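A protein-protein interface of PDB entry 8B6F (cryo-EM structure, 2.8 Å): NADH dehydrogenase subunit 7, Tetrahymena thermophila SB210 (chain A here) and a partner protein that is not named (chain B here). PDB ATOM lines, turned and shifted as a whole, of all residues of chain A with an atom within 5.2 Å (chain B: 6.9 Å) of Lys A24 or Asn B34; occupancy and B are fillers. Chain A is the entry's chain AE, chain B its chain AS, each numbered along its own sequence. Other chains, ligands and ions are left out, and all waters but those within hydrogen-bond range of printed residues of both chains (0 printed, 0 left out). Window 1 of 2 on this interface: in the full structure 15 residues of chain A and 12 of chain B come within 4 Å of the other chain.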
ATOM      1  N   LYS A  21      11.850  25.997  -3.765  1.00  0.00           N
ATOM      2  CA  LYS A  21      11.512  27.166  -2.966  1.00  0.00           C
ATOM      3  C   LYS A  21      12.099  28.416  -3.603  1.00  0.00           C
ATOM      4  O   LYS A  21      13.263  28.754  -3.364  1.00  0.00           O
ATOM      5  CB  LYS A  21      12.024  27.017  -1.532  1.00  0.00           C
ATOM      6  CG  LYS A  21      11.432  25.847  -0.768  1.00  0.00           C
ATOM      7  CD  LYS A  21       9.935  26.004  -0.574  1.00  0.00           C
ATOM      8  CE  LYS A  21       9.379  24.893   0.298  1.00  0.00           C
ATOM      9  NZ  LYS A  21       7.901  24.983   0.417  1.00  0.00           N
ATOM     10  N   GLN A  22      11.309  29.105  -4.417  1.00  0.00           N
ATOM     11  CA  GLN A  22      11.752  30.326  -5.072  1.00  0.00           C
ATOM     12  C   GLN A  22      11.628  31.550  -4.176  1.00  0.00           C
ATOM     13  O   GLN A  22      11.787  32.675  -4.660  1.00  0.00           O
ATOM     14  CB  GLN A  22      10.960  30.540  -6.363  1.00  0.00           C
ATOM     15  CG  GLN A  22      11.250  29.503  -7.433  1.00  0.00           C
ATOM     16  CD  GLN A  22      10.301  29.601  -8.607  1.00  0.00           C
ATOM     17  OE1 GLN A  22       9.094  29.754  -8.430  1.00  0.00           O
ATOM     18  NE2 GLN A  22      10.843  29.526  -9.815  1.00  0.00           N
ATOM     19  N   ILE A  23      11.356  31.356  -2.885  1.00  0.00           N
ATOM     20  CA  ILE A  23      11.132  32.445  -1.950  1.00  0.00           C
ATOM     21  C   ILE A  23      11.912  32.161  -0.676  1.00  0.00           C
ATOM     22  O   ILE A  23      12.223  31.013  -0.353  1.00  0.00           O
ATOM     23  CB  ILE A  23       9.630  32.626  -1.637  1.00  0.00           C
ATOM     24  CG1 ILE A  23       9.410  33.844  -0.742  1.00  0.00           C
ATOM     25  CG2 ILE A  23       9.071  31.367  -0.981  1.00  0.00           C
ATOM     26  CD1 ILE A  23       7.962  34.197  -0.535  1.00  0.00           C
ATOM     27  N   LYS A  24      12.234  33.229   0.050  1.00  0.00           N
ATOM     28  CA  LYS A  24      12.845  33.113   1.368  1.00  0.00           C
ATOM     29  C   LYS A  24      11.724  32.945   2.388  1.00  0.00           C
ATOM     30  O   LYS A  24      11.020  33.905   2.713  1.00  0.00           O
ATOM     31  CB  LYS A  24      13.699  34.341   1.674  1.00  0.00           C
ATOM     32  CG  LYS A  24      14.844  34.082   2.639  1.00  0.00           C
ATOM     33  CD  LYS A  24      14.348  33.822   4.049  1.00  0.00           C
ATOM     34  CE  LYS A  24      15.497  33.554   5.001  1.00  0.00           C
ATOM     35  NZ  LYS A  24      16.201  32.288   4.677  1.00  0.00           N
ATOM     36  N   THR A  25      11.558  31.723   2.886  1.00  0.00           N
ATOM     37  CA  THR A  25      10.455  31.424   3.785  1.00  0.00           C
ATOM     38  C   THR A  25      10.611  32.161   5.110  1.00  0.00           C
ATOM     39  O   THR A  25      11.719  32.485   5.542  1.00  0.00           O
ATOM     40  CB  THR A  25      10.373  29.919   4.036  1.00  0.00           C
ATOM     41  OG1 THR A  25      11.609  29.458   4.598  1.00  0.00           O
ATOM     42  CG2 THR A  25      10.103  29.177   2.737  1.00  0.00           C
ATOM     43  N   MET A  26       9.478  32.430   5.756  1.00  0.00           N
ATOM     44  CA  MET A  26       9.469  33.105   7.048  1.00  0.00           C
ATOM     45  C   MET A  26       9.671  32.074   8.150  1.00  0.00           C
ATOM     46  O   MET A  26       8.812  31.216   8.371  1.00  0.00           O
ATOM     47  CB  MET A  26       8.159  33.859   7.257  1.00  0.00           C
ATOM     48  CG  MET A  26       8.173  35.281   6.739  1.00  0.00           C
ATOM     49  SD  MET A  26       6.670  36.175   7.168  1.00  0.00           S
ATOM     50  CE  MET A  26       7.093  37.818   6.602  1.00  0.00           C
ATOM     51  N   ASN A  27      10.802  32.156   8.840  1.00  0.00           N
ATOM     52  CA  ASN A  27      11.105  31.282   9.970  1.00  0.00           C
ATOM     53  C   ASN A  27      10.771  32.048  11.245  1.00  0.00           C
ATOM     54  O   ASN A  27      11.588  32.823  11.748  1.00  0.00           O
ATOM     55  CB  ASN A  27      12.562  30.845   9.937  1.00  0.00           C
ATOM     56  CG  ASN A  27      12.902  30.041   8.699  1.00  0.00           C
ATOM     57  OD1 ASN A  27      12.033  29.415   8.095  1.00  0.00           O
ATOM     58  ND2 ASN A  27      14.171  30.055   8.317  1.00  0.00           N
ATOM     59  N   TYR B   4      18.364  19.091   5.076  1.00  0.00           N
ATOM     60  CA  TYR B   4      18.731  20.461   5.414  1.00  0.00           C
ATOM     61  C   TYR B   4      20.013  20.887   4.711  1.00  0.00           C
ATOM     62  O   TYR B   4      20.185  22.070   4.397  1.00  0.00           O
ATOM     63  CB  TYR B   4      18.883  20.610   6.926  1.00  0.00           C
ATOM     64  CG  TYR B   4      19.294  21.998   7.346  1.00  0.00           C
ATOM     65  CD1 TYR B   4      18.392  23.051   7.305  1.00  0.00           C
ATOM     66  CD2 TYR B   4      20.583  22.256   7.785  1.00  0.00           C
ATOM     67  CE1 TYR B   4      18.764  24.323   7.688  1.00  0.00           C
ATOM     68  CE2 TYR B   4      20.965  23.524   8.170  1.00  0.00           C
ATOM     69  CZ  TYR B   4      20.050  24.553   8.119  1.00  0.00           C
ATOM     70  OH  TYR B   4      20.428  25.817   8.500  1.00  0.00           O
ATOM     71  N   SER B   8      19.626  22.159  -2.772  1.00  0.00           N
ATOM     72  CA  SER B   8      18.469  22.977  -3.103  1.00  0.00           C
ATOM     73  C   SER B   8      17.941  23.761  -1.911  1.00  0.00           C
ATOM     74  O   SER B   8      16.938  24.466  -2.047  1.00  0.00           O
ATOM     75  CB  SER B   8      17.350  22.100  -3.671  1.00  0.00           C
ATOM     76  OG  SER B   8      17.744  21.493  -4.890  1.00  0.00           O
ATOM     77  N   ASN B   9      18.590  23.662  -0.753  1.00  0.00           N
ATOM     78  CA  ASN B   9      18.182  24.389   0.439  1.00  0.00           C
ATOM     79  C   ASN B   9      18.860  25.749   0.549  1.00  0.00           C
ATOM     80  O   ASN B   9      18.877  26.341   1.632  1.00  0.00           O
ATOM     81  CB  ASN B   9      18.473  23.551   1.685  1.00  0.00           C
ATOM     82  CG  ASN B   9      17.790  24.088   2.924  1.00  0.00           C
ATOM     83  OD1 ASN B   9      16.801  24.813   2.836  1.00  0.00           O
ATOM     84  ND2 ASN B   9      18.313  23.734   4.089  1.00  0.00           N
ATOM     85  N   THR B  10      19.424  26.249  -0.546  1.00  0.00           N
ATOM     86  CA  THR B  10      20.104  27.534  -0.526  1.00  0.00           C
ATOM     87  C   THR B  10      19.098  28.679  -0.479  1.00  0.00           C
ATOM     88  O   THR B  10      17.947  28.544  -0.902  1.00  0.00           O
ATOM     89  CB  THR B  10      20.990  27.684  -1.762  1.00  0.00           C
ATOM     90  OG1 THR B  10      20.183  27.620  -2.946  1.00  0.00           O
ATOM     91  CG2 THR B  10      22.036  26.585  -1.814  1.00  0.00           C
ATOM     92  N   ILE B  11      19.543  29.814   0.050  1.00  0.00           N
ATOM     93  CA  ILE B  11      18.739  31.033   0.061  1.00  0.00           C
ATOM     94  C   ILE B  11      18.868  31.691  -1.308  1.00  0.00           C
ATOM     95  O   ILE B  11      19.993  31.985  -1.739  1.00  0.00           O
ATOM     96  CB  ILE B  11      19.178  31.989   1.181  1.00  0.00           C
ATOM     97  CG1 ILE B  11      19.065  31.295   2.542  1.00  0.00           C
ATOM     98  CG2 ILE B  11      18.335  33.258   1.152  1.00  0.00           C
ATOM     99  CD1 ILE B  11      19.557  32.128   3.710  1.00  0.00           C
ATOM    100  N   PRO B  12      17.773  31.944  -2.027  1.00  0.00           N
ATOM    101  CA  PRO B  12      17.900  32.578  -3.345  1.00  0.00           C
ATOM    102  C   PRO B  12      18.586  33.931  -3.252  1.00  0.00           C
ATOM    103  O   PRO B  12      18.380  34.689  -2.302  1.00  0.00           O
ATOM    104  CB  PRO B  12      16.448  32.717  -3.815  1.00  0.00           C
ATOM    105  CG  PRO B  12      15.697  31.698  -3.049  1.00  0.00           C
ATOM    106  CD  PRO B  12      16.374  31.607  -1.717  1.00  0.00           C
ATOM    107  N   ASN B  27      24.643  29.598  -1.592  1.00  0.00           N
ATOM    108  CA  ASN B  27      25.552  29.274  -0.501  1.00  0.00           C
ATOM    109  C   ASN B  27      24.767  28.626   0.631  1.00  0.00           C
ATOM    110  O   ASN B  27      23.809  29.211   1.145  1.00  0.00           O
ATOM    111  CB  ASN B  27      26.272  30.525  -0.002  1.00  0.00           C
ATOM    112  CG  ASN B  27      27.154  30.249   1.196  1.00  0.00           C
ATOM    113  OD1 ASN B  27      27.474  29.102   1.492  1.00  0.00           O
ATOM    114  ND2 ASN B  27      27.557  31.305   1.889  1.00  0.00           N
ATOM    115  N   ASN B  28      25.180  27.421   1.012  1.00  0.00           N
ATOM    116  CA  ASN B  28      24.567  26.710   2.123  1.00  0.00           C
ATOM    117  C   ASN B  28      25.601  26.081   3.045  1.00  0.00           C
ATOM    118  O   ASN B  28      25.214  25.434   4.022  1.00  0.00           O
ATOM    119  CB  ASN B  28      23.617  25.624   1.592  1.00  0.00           C
ATOM    120  CG  ASN B  28      22.710  25.063   2.661  1.00  0.00           C
ATOM    121  OD1 ASN B  28      22.551  25.650   3.730  1.00  0.00           O
ATOM    122  ND2 ASN B  28      22.096  23.923   2.373  1.00  0.00           N
ATOM    123  N   ARG B  32      23.466  29.363   7.158  1.00  0.00           N
ATOM    124  CA  ARG B  32      22.323  28.480   7.333  1.00  0.00           C
ATOM    125  C   ARG B  32      21.488  28.422   6.059  1.00  0.00           C
ATOM    126  O   ARG B  32      21.447  29.368   5.269  1.00  0.00           O
ATOM    127  CB  ARG B  32      21.458  28.941   8.506  1.00  0.00           C
ATOM    128  CG  ARG B  32      21.008  30.388   8.432  1.00  0.00           C
ATOM    129  CD  ARG B  32      19.863  30.646   9.398  1.00  0.00           C
ATOM    130  NE  ARG B  32      19.603  32.069   9.570  1.00  0.00           N
ATOM    131  CZ  ARG B  32      20.103  32.819  10.543  1.00  0.00           C
ATOM    132  NH1 ARG B  32      20.900  32.314  11.470  1.00  0.00           N
ATOM    133  NH2 ARG B  32      19.800  34.113  10.585  1.00  0.00           N
ATOM    134  N   GLY B  33      20.811  27.295   5.870  1.00  0.00           N
ATOM    135  CA  GLY B  33      20.011  27.081   4.684  1.00  0.00           C
ATOM    136  C   GLY B  33      18.719  27.875   4.715  1.00  0.00           C
ATOM    137  O   GLY B  33      18.438  28.655   5.625  1.00  0.00           O
ATOM    138  N   ASN B  34      17.911  27.663   3.676  1.00  0.00           N
ATOM    139  CA  ASN B  34      16.665  28.407   3.539  1.00  0.00           C
ATOM    140  C   ASN B  34      15.559  27.812   4.405  1.00  0.00           C
ATOM    141  O   ASN B  34      14.941  28.520   5.207  1.00  0.00           O
ATOM    142  CB  ASN B  34      16.239  28.436   2.071  1.00  0.00           C
ATOM    143  CG  ASN B  34      15.105  29.400   1.814  1.00  0.00           C
ATOM    144  OD1 ASN B  34      14.838  30.289   2.619  1.00  0.00           O
ATOM    145  ND2 ASN B  34      14.429  29.231   0.686  1.00  0.00           N
ATOM    146  N   GLU B  35      15.300  26.517   4.261  1.00  0.00           N
ATOM    147  CA  GLU B  35      14.277  25.840   5.045  1.00  0.00           C
ATOM    148  C   GLU B  35      14.871  25.312   6.346  1.00  0.00           C
ATOM    149  O   GLU B  35      16.040  24.920   6.403  1.00  0.00           O
ATOM    150  CB  GLU B  35      13.662  24.687   4.252  1.00  0.00           C
ATOM    151  CG  GLU B  35      13.161  25.084   2.873  1.00  0.00           C
ATOM    152  CD  GLU B  35      12.436  23.952   2.169  1.00  0.00           C
ATOM    153  OE1 GLU B  35      11.598  23.290   2.816  1.00  0.00           O
ATOM    154  OE2 GLU B  35      12.707  23.717   0.973  1.00  0.00           O
ATOM    155  N   ILE B  36      14.050  25.299   7.394  1.00  0.00           N
ATOM    156  CA  ILE B  36      14.492  24.841   8.707  1.00  0.00           C
ATOM    157  C   ILE B  36      14.693  23.333   8.672  1.00  0.00           C
ATOM    158  O   ILE B  36      14.240  22.655   7.745  1.00  0.00           O
ATOM    159  CB  ILE B  36      13.493  25.236   9.811  1.00  0.00           C
ATOM    160  CG1 ILE B  36      12.127  24.587   9.560  1.00  0.00           C
ATOM    161  CG2 ILE B  36      13.375  26.753   9.882  1.00  0.00           C
ATOM    162  CD1 ILE B  36      11.110  24.841  10.655  1.00  0.00           C
ATOM    163  N   MET B 121      21.213  28.654  14.116  1.00  0.00           N
ATOM    164  CA  MET B 121      19.843  29.140  14.143  1.00  0.00           C
ATOM    165  C   MET B 121      19.536  30.001  15.360  1.00  0.00           C
ATOM    166  O   MET B 121      18.372  30.353  15.572  1.00  0.00           O
ATOM    167  CB  MET B 121      18.873  27.958  14.097  1.00  0.00           C
ATOM    168  CG  MET B 121      18.736  27.322  12.728  1.00  0.00           C
ATOM    169  SD  MET B 121      17.962  28.414  11.522  1.00  0.00           S
ATOM    170  CE  MET B 121      17.880  27.335  10.095  1.00  0.00           C
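O of Asn B9 lies within hydrogen-bond range of N of Asn B34 (2.6 Å).
The backbone NH (N) of Glu B35 sits at hydrogen-bond distance from the side-chain amide oxygen (OD1) of Asn B9, 2.7 Å away.
Printed residues of chain B within 4 Å of Lys A24: Ile B11 (3.5 Å) and Asn B34 (3.2 Å).
Of the printed residues of chain A, Asn B34 touches Lys A21 (3.95 Å), Ile A23 (3.0 Å), Lys A24 (3.2 Å), Thr A25 (3.5 Å) and Asn A27 (3.6 Å).
Printed residues of chain A within 4 Å of Glu B35: Lys A21 (3.0 Å).
Of the printed residues of chain B, Lys A21 touches Pro B12 (3.8 Å), Asn B34 (3.95 Å) and Glu B35 (3.0 Å).
Asn B28 touches none of the printed residues of chain A.
Ser B8 touches none of the printed residues of chain A.
CG of Pro B12 touches O of Lys A21 (3.8 Å).
Asn B34 touches Lys A21 (ND2 to CB, 3.95 Å).
OE2 of Glu B35 touches CG of Lys A21 (3.0 Å).
Lys A24 touches Ile B11.
Thr A25 touches Asn B34.
Asn A27 touches Asn B34 (ND2 to O, 3.6 Å).
OD1 of Asn A27 touches CG2 of Ile B36 (3.5 Å).
The side-chain amide nitrogen of Asn B34 is in hydrogen-bond range of the backbone carbonyl oxygen of Ile A23, at 3.0 Å.
The side-chain amino group (NZ) of Lys A24 is in hydrogen-bond range of the side-chain amide oxygen (OD1) of Asn B34.
Hydrophobic or aromatic side chains of chain B that line the printed part of chain A: Ile B11, Pro B12 and Ile B36.
Among the printed residues, 9 pairs touch across the chains.
Among the printed residues, no Asp or Glu carboxylate lies within 4 Å of a Lys or Arg side-chain nitrogen of the other chain.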
